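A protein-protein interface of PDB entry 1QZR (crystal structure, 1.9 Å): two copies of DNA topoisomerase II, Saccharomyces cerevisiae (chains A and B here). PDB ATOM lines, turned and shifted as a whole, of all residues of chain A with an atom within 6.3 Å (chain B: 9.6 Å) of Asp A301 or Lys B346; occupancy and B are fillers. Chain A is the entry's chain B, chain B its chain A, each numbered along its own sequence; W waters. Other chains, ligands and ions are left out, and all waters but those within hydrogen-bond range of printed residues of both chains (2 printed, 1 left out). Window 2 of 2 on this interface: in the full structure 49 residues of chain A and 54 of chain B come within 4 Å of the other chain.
Water W2 bridges the side-chain amino group (NZ) of Lys B346 (2.9 Å) and the side-chain amide nitrogen (ND2) of Asn A353 (3.4 Å).
Water W1 lies within hydrogen-bond range of the backbone NH of Phe B348 (3.0 Å), the backbone carbonyl oxygen of Ile A302 (3.0 Å) and the backbone NH of Ser B347 (3.3 Å).
NZ of Lys B346 is in hydrogen-bond range of OD1 of Asn A353 (3.4 Å).
Among the printed residues, pairs that only touch across the chains: Ile A302 with Phe B348 (3.2 Å), Asn A352 with Phe B348 (3.7 Å), Asp A301 with Lys B346 (3.8 Å) and Asn A352 with Asn B352 (3.97 Å).
The side-chain amide oxygen of Asn A353 is in hydrogen-bond range of the guanidinium group of Arg A404 (2.9 Å).
O of Phe B348 sits at hydrogen-bond distance from ND2 of Asn B352 (2.7 Å).
N of Ser A300 sits at hydrogen-bond distance from O of Asn A353 (2.9 Å).
N of Lys B346 sits at hydrogen-bond distance from OE1 of Gln B349, at 2.9 Å.
OD1 of Asp A301 lies within salt-bridge range of NH2 of Arg A404 (3.2 Å).
Ser A300 touches none of the printed residues of chain B.
Printed residues of chain B within 4 Å of Asp A301: Lys B346.
Of the printed residues of chain B, Ile A302 touches Phe B348 (3.2 Å).
Of the printed residues of chain B, Asn A353 touches Lys B346 (3.4 Å).
Ile B408 touches none of the printed residues of chain A.
The nearest residue of chain B that does not touch Asp A301 is Phe B348 (6.0 Å).
The nearest printed residue of chain A that does not touch Lys B346 is Arg A404 (4.001 Å).
Of the 10 printed residues of chain A, 4 touch a printed residue of chain B.
Among the printed residues, no Asp or Glu carboxylate lies within 4 Å of a Lys or Arg side-chain nitrogen of the other chain.
Asn A352 touches its own counterpart, Asn B352.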
ATOM      1  N   LEU A 263      28.723 -31.516 -10.622  1.00  0.00           N
ATOM      2  CA  LEU A 263      27.738 -31.417 -11.697  1.00  0.00           C
ATOM      3  C   LEU A 263      26.531 -32.326 -11.463  1.00  0.00           C
ATOM      4  O   LEU A 263      25.399 -31.945 -11.756  1.00  0.00           O
ATOM      5  CB  LEU A 263      28.378 -31.711 -13.059  1.00  0.00           C
ATOM      6  CG  LEU A 263      29.309 -30.627 -13.613  1.00  0.00           C
ATOM      7  CD1 LEU A 263      30.093 -31.138 -14.802  1.00  0.00           C
ATOM      8  CD2 LEU A 263      28.535 -29.369 -13.983  1.00  0.00           C
ATOM      9  N   LYS A 265      25.456 -33.137  -8.581  1.00  0.00           N
ATOM     10  CA  LYS A 265      24.791 -32.618  -7.386  1.00  0.00           C
ATOM     11  C   LYS A 265      23.648 -31.683  -7.749  1.00  0.00           C
ATOM     12  O   LYS A 265      22.481 -32.001  -7.513  1.00  0.00           O
ATOM     13  CB  LYS A 265      25.790 -31.910  -6.477  1.00  0.00           C
ATOM     14  N   VAL A 299      25.449 -30.749 -19.111  1.00  0.00           N
ATOM     15  CA  VAL A 299      24.384 -29.754 -19.069  1.00  0.00           C
ATOM     16  C   VAL A 299      24.678 -28.680 -18.016  1.00  0.00           C
ATOM     17  O   VAL A 299      25.083 -28.988 -16.883  1.00  0.00           O
ATOM     18  CB  VAL A 299      23.003 -30.407 -18.803  1.00  0.00           C
ATOM     19  CG1 VAL A 299      21.887 -29.346 -18.792  1.00  0.00           C
ATOM     20  CG2 VAL A 299      22.706 -31.442 -19.864  1.00  0.00           C
ATOM     21  N   SER A 300      24.492 -27.421 -18.404  1.00  0.00           N
ATOM     22  CA  SER A 300      24.723 -26.301 -17.501  1.00  0.00           C
ATOM     23  C   SER A 300      23.408 -25.844 -16.884  1.00  0.00           C
ATOM     24  O   SER A 300      22.377 -25.803 -17.568  1.00  0.00           O
ATOM     25  CB  SER A 300      25.369 -25.150 -18.253  1.00  0.00           C
ATOM     26  OG  SER A 300      25.948 -24.238 -17.351  1.00  0.00           O
ATOM     27  N   ASP A 301      23.451 -25.495 -15.602  1.00  0.00           N
ATOM     28  CA  ASP A 301      22.237 -25.141 -14.855  1.00  0.00           C
ATOM     29  C   ASP A 301      21.902 -23.646 -14.869  1.00  0.00           C
ATOM     30  O   ASP A 301      20.723 -23.275 -14.790  1.00  0.00           O
ATOM     31  CB  ASP A 301      22.315 -25.660 -13.407  1.00  0.00           C
ATOM     32  CG  ASP A 301      21.937 -27.135 -13.292  1.00  0.00           C
ATOM     33  OD1 ASP A 301      21.043 -27.591 -14.046  1.00  0.00           O
ATOM     34  OD2 ASP A 301      22.485 -27.921 -12.482  1.00  0.00           O
ATOM     35  N   ILE A 302      22.925 -22.797 -14.971  1.00  0.00           N
ATOM     36  CA  ILE A 302      22.724 -21.342 -14.940  1.00  0.00           C
ATOM     37  C   ILE A 302      22.947 -20.671 -16.303  1.00  0.00           C
ATOM     38  O   ILE A 302      22.050 -20.007 -16.825  1.00  0.00           O
ATOM     39  CB  ILE A 302      23.613 -20.662 -13.851  1.00  0.00           C
ATOM     40  CG1 ILE A 302      23.297 -21.213 -12.451  1.00  0.00           C
ATOM     41  CG2 ILE A 302      23.434 -19.139 -13.882  1.00  0.00           C
ATOM     42  CD1 ILE A 302      22.000 -20.682 -11.836  1.00  0.00           C
ATOM     43  N   SER A 303      24.147 -20.822 -16.859  1.00  0.00           N
ATOM     44  CA  SER A 303      24.483 -20.210 -18.141  1.00  0.00           C
ATOM     45  C   SER A 303      25.607 -20.976 -18.827  1.00  0.00           C
ATOM     46  O   SER A 303      26.078 -21.992 -18.310  1.00  0.00           O
ATOM     47  CB  SER A 303      24.863 -18.746 -17.953  1.00  0.00           C
ATOM     48  OG  SER A 303      26.033 -18.641 -17.166  1.00  0.00           O
ATOM     49  N   ASN A 352      23.377 -21.461 -23.721  1.00  0.00           N
ATOM     50  CA  ASN A 352      23.388 -21.232 -22.285  1.00  0.00           C
ATOM     51  C   ASN A 352      22.977 -22.415 -21.420  1.00  0.00           C
ATOM     52  O   ASN A 352      22.966 -22.322 -20.193  1.00  0.00           O
ATOM     53  CB  ASN A 352      22.625 -19.971 -21.941  1.00  0.00           C
ATOM     54  CG  ASN A 352      23.457 -18.738 -22.186  1.00  0.00           C
ATOM     55  OD1 ASN A 352      24.366 -18.451 -21.430  1.00  0.00           O
ATOM     56  ND2 ASN A 352      23.192 -18.046 -23.290  1.00  0.00           N
ATOM     57  N   ASN A 353      22.648 -23.520 -22.068  1.00  0.00           N
ATOM     58  CA  ASN A 353      22.452 -24.772 -21.371  1.00  0.00           C
ATOM     59  C   ASN A 353      23.654 -25.713 -21.505  1.00  0.00           C
ATOM     60  O   ASN A 353      23.587 -26.857 -21.068  1.00  0.00           O
ATOM     61  CB  ASN A 353      21.166 -25.450 -21.867  1.00  0.00           C
ATOM     62  CG  ASN A 353      19.919 -24.796 -21.310  1.00  0.00           C
ATOM     63  OD1 ASN A 353      19.521 -25.061 -20.181  1.00  0.00           O
ATOM     64  ND2 ASN A 353      19.319 -23.912 -22.084  1.00  0.00           N
ATOM     65  N   ARG A 404      14.763 -29.311 -22.248  1.00  0.00           N
ATOM     66  CA  ARG A 404      14.588 -27.879 -22.015  1.00  0.00           C
ATOM     67  C   ARG A 404      14.274 -27.120 -23.313  1.00  0.00           C
ATOM     68  O   ARG A 404      13.372 -26.280 -23.342  1.00  0.00           O
ATOM     69  CB  ARG A 404      15.826 -27.282 -21.327  1.00  0.00           C
ATOM     70  CG  ARG A 404      15.946 -27.626 -19.848  1.00  0.00           C
ATOM     71  CD  ARG A 404      17.213 -27.081 -19.201  1.00  0.00           C
ATOM     72  NE  ARG A 404      17.720 -27.930 -18.127  1.00  0.00           N
ATOM     73  CZ  ARG A 404      18.890 -27.743 -17.518  1.00  0.00           C
ATOM     74  NH1 ARG A 404      19.676 -26.739 -17.880  1.00  0.00           N
ATOM     75  NH2 ARG A 404      19.279 -28.561 -16.542  1.00  0.00           N
ATOM     76  N   VAL B 330      19.285  -6.412 -15.277  1.00  0.00           N
ATOM     77  CA  VAL B 330      18.825  -7.793 -15.156  1.00  0.00           C
ATOM     78  C   VAL B 330      18.286  -8.109 -13.752  1.00  0.00           C
ATOM     79  O   VAL B 330      17.217  -8.721 -13.611  1.00  0.00           O
ATOM     80  CB  VAL B 330      19.932  -8.808 -15.541  1.00  0.00           C
ATOM     81  CG1 VAL B 330      19.535 -10.228 -15.121  1.00  0.00           C
ATOM     82  CG2 VAL B 330      20.204  -8.758 -17.053  1.00  0.00           C
ATOM     83  N   LYS B 331      19.023  -7.692 -12.724  1.00  0.00           N
ATOM     84  CA  LYS B 331      18.598  -7.919 -11.342  1.00  0.00           C
ATOM     85  C   LYS B 331      17.258  -7.244 -11.038  1.00  0.00           C
ATOM     86  O   LYS B 331      16.372  -7.849 -10.432  1.00  0.00           O
ATOM     87  CB  LYS B 331      19.673  -7.439 -10.360  1.00  0.00           C
ATOM     88  CG  LYS B 331      19.410  -7.810  -8.912  1.00  0.00           C
ATOM     89  CD  LYS B 331      20.428  -7.139  -7.988  1.00  0.00           C
ATOM     90  CE  LYS B 331      20.121  -7.423  -6.529  1.00  0.00           C
ATOM     91  NZ  LYS B 331      21.104  -6.750  -5.621  1.00  0.00           N
ATOM     92  N   ILE B 333      14.887  -6.126 -13.243  1.00  0.00           N
ATOM     93  CA  ILE B 333      13.813  -6.751 -14.025  1.00  0.00           C
ATOM     94  C   ILE B 333      13.381  -8.069 -13.389  1.00  0.00           C
ATOM     95  O   ILE B 333      12.181  -8.316 -13.204  1.00  0.00           O
ATOM     96  CB  ILE B 333      14.229  -6.951 -15.506  1.00  0.00           C
ATOM     97  CG1 ILE B 333      14.243  -5.603 -16.234  1.00  0.00           C
ATOM     98  CG2 ILE B 333      13.291  -7.932 -16.214  1.00  0.00           C
ATOM     99  CD1 ILE B 333      14.896  -5.653 -17.585  1.00  0.00           C
ATOM    100  N   SER B 334      14.358  -8.903 -13.043  1.00  0.00           N
ATOM    101  CA  SER B 334      14.083 -10.200 -12.435  1.00  0.00           C
ATOM    102  C   SER B 334      13.218 -10.066 -11.172  1.00  0.00           C
ATOM    103  O   SER B 334      12.258 -10.820 -10.984  1.00  0.00           O
ATOM    104  CB  SER B 334      15.389 -10.934 -12.129  1.00  0.00           C
ATOM    105  OG  SER B 334      15.132 -12.271 -11.748  1.00  0.00           O
ATOM    106  N   LEU B 337       9.728  -9.340 -12.120  1.00  0.00           N
ATOM    107  CA  LEU B 337       9.156 -10.573 -12.659  1.00  0.00           C
ATOM    108  C   LEU B 337       8.748 -11.551 -11.556  1.00  0.00           C
ATOM    109  O   LEU B 337       7.670 -12.154 -11.613  1.00  0.00           O
ATOM    110  CB  LEU B 337      10.137 -11.242 -13.622  1.00  0.00           C
ATOM    111  CG  LEU B 337       9.933 -10.939 -15.107  1.00  0.00           C
ATOM    112  CD1 LEU B 337      11.240 -11.099 -15.860  1.00  0.00           C
ATOM    113  CD2 LEU B 337       8.854 -11.841 -15.697  1.00  0.00           C
ATOM    114  N   VAL B 345      12.339 -16.317 -14.352  1.00  0.00           N
ATOM    115  CA  VAL B 345      13.070 -16.675 -15.563  1.00  0.00           C
ATOM    116  C   VAL B 345      14.572 -16.644 -15.294  1.00  0.00           C
ATOM    117  O   VAL B 345      15.012 -16.028 -14.330  1.00  0.00           O
ATOM    118  CB  VAL B 345      12.697 -15.743 -16.745  1.00  0.00           C
ATOM    119  CG1 VAL B 345      11.190 -15.505 -16.777  1.00  0.00           C
ATOM    120  CG2 VAL B 345      13.449 -14.429 -16.667  1.00  0.00           C
ATOM    121  N   LYS B 346      15.357 -17.316 -16.133  1.00  0.00           N
ATOM    122  CA  LYS B 346      16.816 -17.296 -15.976  1.00  0.00           C
ATOM    123  C   LYS B 346      17.380 -15.934 -16.399  1.00  0.00           C
ATOM    124  O   LYS B 346      16.854 -15.289 -17.310  1.00  0.00           O
ATOM    125  CB  LYS B 346      17.472 -18.434 -16.773  1.00  0.00           C
ATOM    126  CG  LYS B 346      17.124 -19.853 -16.267  1.00  0.00           C
ATOM    127  CD  LYS B 346      18.138 -20.890 -16.763  1.00  0.00           C
ATOM    128  CE  LYS B 346      17.595 -22.316 -16.672  1.00  0.00           C
ATOM    129  NZ  LYS B 346      17.939 -23.135 -17.886  1.00  0.00           N
ATOM    130  N   SER B 347      18.440 -15.504 -15.725  1.00  0.00           N
ATOM    131  CA  SER B 347      19.074 -14.221 -16.000  1.00  0.00           C
ATOM    132  C   SER B 347      19.581 -14.083 -17.437  1.00  0.00           C
ATOM    133  O   SER B 347      19.464 -13.028 -18.039  1.00  0.00           O
ATOM    134  CB  SER B 347      20.208 -13.966 -15.012  1.00  0.00           C
ATOM    135  OG  SER B 347      19.676 -13.771 -13.712  1.00  0.00           O
ATOM    136  N   PHE B 348      20.119 -15.150 -18.001  1.00  0.00           N
ATOM    137  CA  PHE B 348      20.588 -15.064 -19.381  1.00  0.00           C
ATOM    138  C   PHE B 348      19.432 -14.806 -20.380  1.00  0.00           C
ATOM    139  O   PHE B 348      19.651 -14.287 -21.470  1.00  0.00           O
ATOM    140  CB  PHE B 348      21.398 -16.310 -19.757  1.00  0.00           C
ATOM    141  CG  PHE B 348      20.561 -17.514 -20.097  1.00  0.00           C
ATOM    142  CD1 PHE B 348      19.874 -17.587 -21.308  1.00  0.00           C
ATOM    143  CD2 PHE B 348      20.505 -18.597 -19.234  1.00  0.00           C
ATOM    144  CE1 PHE B 348      19.127 -18.721 -21.643  1.00  0.00           C
ATOM    145  CE2 PHE B 348      19.765 -19.725 -19.554  1.00  0.00           C
ATOM    146  CZ  PHE B 348      19.063 -19.785 -20.757  1.00  0.00           C
ATOM    147  N   GLN B 349      18.218 -15.194 -20.001  1.00  0.00           N
ATOM    148  CA  GLN B 349      17.037 -14.983 -20.850  1.00  0.00           C
ATOM    149  C   GLN B 349      16.680 -13.490 -20.956  1.00  0.00           C
ATOM    150  O   GLN B 349      16.329 -12.994 -22.037  1.00  0.00           O
ATOM    151  CB  GLN B 349      15.850 -15.801 -20.331  1.00  0.00           C
ATOM    152  CG  GLN B 349      15.926 -17.304 -20.718  1.00  0.00           C
ATOM    153  CD  GLN B 349      14.978 -18.196 -19.927  1.00  0.00           C
ATOM    154  OE1 GLN B 349      14.551 -17.847 -18.823  1.00  0.00           O
ATOM    155  NE2 GLN B 349      14.653 -19.362 -20.491  1.00  0.00           N
ATOM    156  N   ILE B 350      16.799 -12.778 -19.841  1.00  0.00           N
ATOM    157  CA  ILE B 350      16.586 -11.329 -19.817  1.00  0.00           C
ATOM    158  C   ILE B 350      17.711 -10.601 -20.522  1.00  0.00           C
ATOM    159  O   ILE B 350      17.475  -9.739 -21.388  1.00  0.00           O
ATOM    160  CB  ILE B 350      16.448 -10.809 -18.357  1.00  0.00           C
ATOM    161  CG1 ILE B 350      15.288 -11.510 -17.634  1.00  0.00           C
ATOM    162  CG2 ILE B 350      16.242  -9.282 -18.345  1.00  0.00           C
ATOM    163  CD1 ILE B 350      15.375 -11.421 -16.108  1.00  0.00           C
ATOM    164  N   LYS B 351      18.942 -10.943 -20.145  1.00  0.00           N
ATOM    165  CA  LYS B 351      20.121 -10.355 -20.757  1.00  0.00           C
ATOM    166  C   LYS B 351      20.101 -10.422 -22.287  1.00  0.00           C
ATOM    167  O   LYS B 351      20.382  -9.426 -22.957  1.00  0.00           O
ATOM    168  CB  LYS B 351      21.391 -11.009 -20.214  1.00  0.00           C
ATOM    169  CG  LYS B 351      22.590 -10.049 -20.208  1.00  0.00           C
ATOM    170  CD  LYS B 351      23.920 -10.777 -20.175  1.00  0.00           C
ATOM    171  CE  LYS B 351      25.047  -9.804 -20.557  1.00  0.00           C
ATOM    172  NZ  LYS B 351      26.331 -10.125 -19.866  1.00  0.00           N
ATOM    173  N   ASN B 352      19.754 -11.586 -22.837  1.00  0.00           N
ATOM    174  CA  ASN B 352      19.834 -11.778 -24.289  1.00  0.00           C
ATOM    175  C   ASN B 352      18.706 -11.161 -25.119  1.00  0.00           C
ATOM    176  O   ASN B 352      18.632 -11.359 -26.350  1.00  0.00           O
ATOM    177  CB  ASN B 352      20.001 -13.252 -24.623  1.00  0.00           C
ATOM    178  CG  ASN B 352      21.414 -13.714 -24.425  1.00  0.00           C
ATOM    179  OD1 ASN B 352      22.287 -13.431 -25.249  1.00  0.00           O
ATOM    180  ND2 ASN B 352      21.674 -14.373 -23.303  1.00  0.00           N
ATOM    181  N   ASN B 353      17.829 -10.418 -24.459  1.00  0.00           N
ATOM    182  CA  ASN B 353      16.833  -9.631 -25.161  1.00  0.00           C
ATOM    183  C   ASN B 353      17.171  -8.127 -25.103  1.00  0.00           C
ATOM    184  O   ASN B 353      16.376  -7.265 -25.496  1.00  0.00           O
ATOM    185  CB  ASN B 353      15.445  -9.931 -24.606  1.00  0.00           C
ATOM    186  CG  ASN B 353      14.858 -11.208 -25.182  1.00  0.00           C
ATOM    187  OD1 ASN B 353      14.269 -11.196 -26.249  1.00  0.00           O
ATOM    188  ND2 ASN B 353      15.067 -12.321 -24.497  1.00  0.00           N
ATOM    189  N   LEU B 401      10.613  -6.616 -24.522  1.00  0.00           N
ATOM    190  CA  LEU B 401      11.397  -7.405 -23.567  1.00  0.00           C
ATOM    191  C   LEU B 401      10.498  -8.020 -22.485  1.00  0.00           C
ATOM    192  O   LEU B 401      10.653  -9.187 -22.131  1.00  0.00           O
ATOM    193  CB  LEU B 401      12.510  -6.562 -22.934  1.00  0.00           C
ATOM    194  CG  LEU B 401      13.463  -7.306 -21.983  1.00  0.00           C
ATOM    195  CD1 LEU B 401      14.876  -6.732 -22.064  1.00  0.00           C
ATOM    196  CD2 LEU B 401      12.952  -7.283 -20.545  1.00  0.00           C
ATOM    197  N   ARG B 404       8.161 -10.826 -23.869  1.00  0.00           N
ATOM    198  CA  ARG B 404       8.950 -12.033 -24.070  1.00  0.00           C
ATOM    199  C   ARG B 404       9.253 -12.767 -22.765  1.00  0.00           C
ATOM    200  O   ARG B 404       9.278 -13.995 -22.733  1.00  0.00           O
ATOM    201  CB  ARG B 404      10.247 -11.703 -24.806  1.00  0.00           C
ATOM    202  CG  ARG B 404      10.056 -11.349 -26.277  1.00  0.00           C
ATOM    203  CD  ARG B 404      11.363 -11.019 -26.981  1.00  0.00           C
ATOM    204  NE  ARG B 404      11.200 -10.125 -28.125  1.00  0.00           N
ATOM    205  CZ  ARG B 404      12.207  -9.512 -28.735  1.00  0.00           C
ATOM    206  NH1 ARG B 404      13.452  -9.688 -28.307  1.00  0.00           N
ATOM    207  NH2 ARG B 404      11.975  -8.719 -29.772  1.00  0.00           N
ATOM    208  N   MET B 405       9.483 -12.017 -21.691  1.00  0.00           N
ATOM    209  CA  MET B 405       9.789 -12.628 -20.405  1.00  0.00           C
ATOM    210  C   MET B 405       8.526 -13.237 -19.770  1.00  0.00           C
ATOM    211  O   MET B 405       8.574 -14.339 -19.222  1.00  0.00           O
ATOM    212  CB  MET B 405      10.473 -11.632 -19.464  1.00  0.00           C
ATOM    213  CG  MET B 405      11.896 -11.187 -19.913  1.00  0.00           C
ATOM    214  SD  MET B 405      13.048 -12.540 -20.378  1.00  0.00           S
ATOM    215  CE  MET B 405      12.912 -12.584 -22.155  1.00  0.00           C
ATOM    216  N   ILE B 408       7.935 -16.596 -21.329  1.00  0.00           N
ATOM    217  CA  ILE B 408       8.796 -17.601 -20.706  1.00  0.00           C
ATOM    218  C   ILE B 408       8.251 -17.987 -19.327  1.00  0.00           C
ATOM    219  O   ILE B 408       8.146 -19.176 -19.002  1.00  0.00           O
ATOM    220  CB  ILE B 408      10.264 -17.110 -20.612  1.00  0.00           C
ATOM    221  CG1 ILE B 408      10.892 -17.021 -22.009  1.00  0.00           C
ATOM    222  CG2 ILE B 408      11.087 -18.041 -19.706  1.00  0.00           C
ATOM    223  CD1 ILE B 408      12.267 -16.331 -22.036  1.00  0.00           C
ATOM    224  N   ALA B 409       7.862 -16.976 -18.549  1.00  0.00           N
ATOM    225  CA  ALA B 409       7.375 -17.164 -17.180  1.00  0.00           C
ATOM    226  C   ALA B 409       6.179 -18.118 -17.054  1.00  0.00           C
ATOM    227  O   ALA B 409       6.216 -19.059 -16.257  1.00  0.00           O
ATOM    228  CB  ALA B 409       7.060 -15.823 -16.540  1.00  0.00           C
ATOM    229  N   ASN B 412       6.994 -21.585 -18.034  1.00  0.00           N
ATOM    230  CA  ASN B 412       7.656 -22.225 -16.895  1.00  0.00           C
ATOM    231  C   ASN B 412       6.667 -22.698 -15.823  1.00  0.00           C
ATOM    232  O   ASN B 412       6.940 -23.663 -15.103  1.00  0.00           O
ATOM    233  CB  ASN B 412       8.696 -21.285 -16.268  1.00  0.00           C
ATOM    234  CG  ASN B 412       9.949 -21.121 -17.128  1.00  0.00           C
ATOM    235  OD1 ASN B 412      10.150 -21.839 -18.108  1.00  0.00           O
ATOM    236  ND2 ASN B 412      10.797 -20.170 -16.754  1.00  0.00           N
HETATM  237  O   HOH W   1      21.213 -17.195 -16.051  1.00  0.00           O
HETATM  238  O   HOH W   2      16.558 -22.775 -20.463  1.00  0.00           O
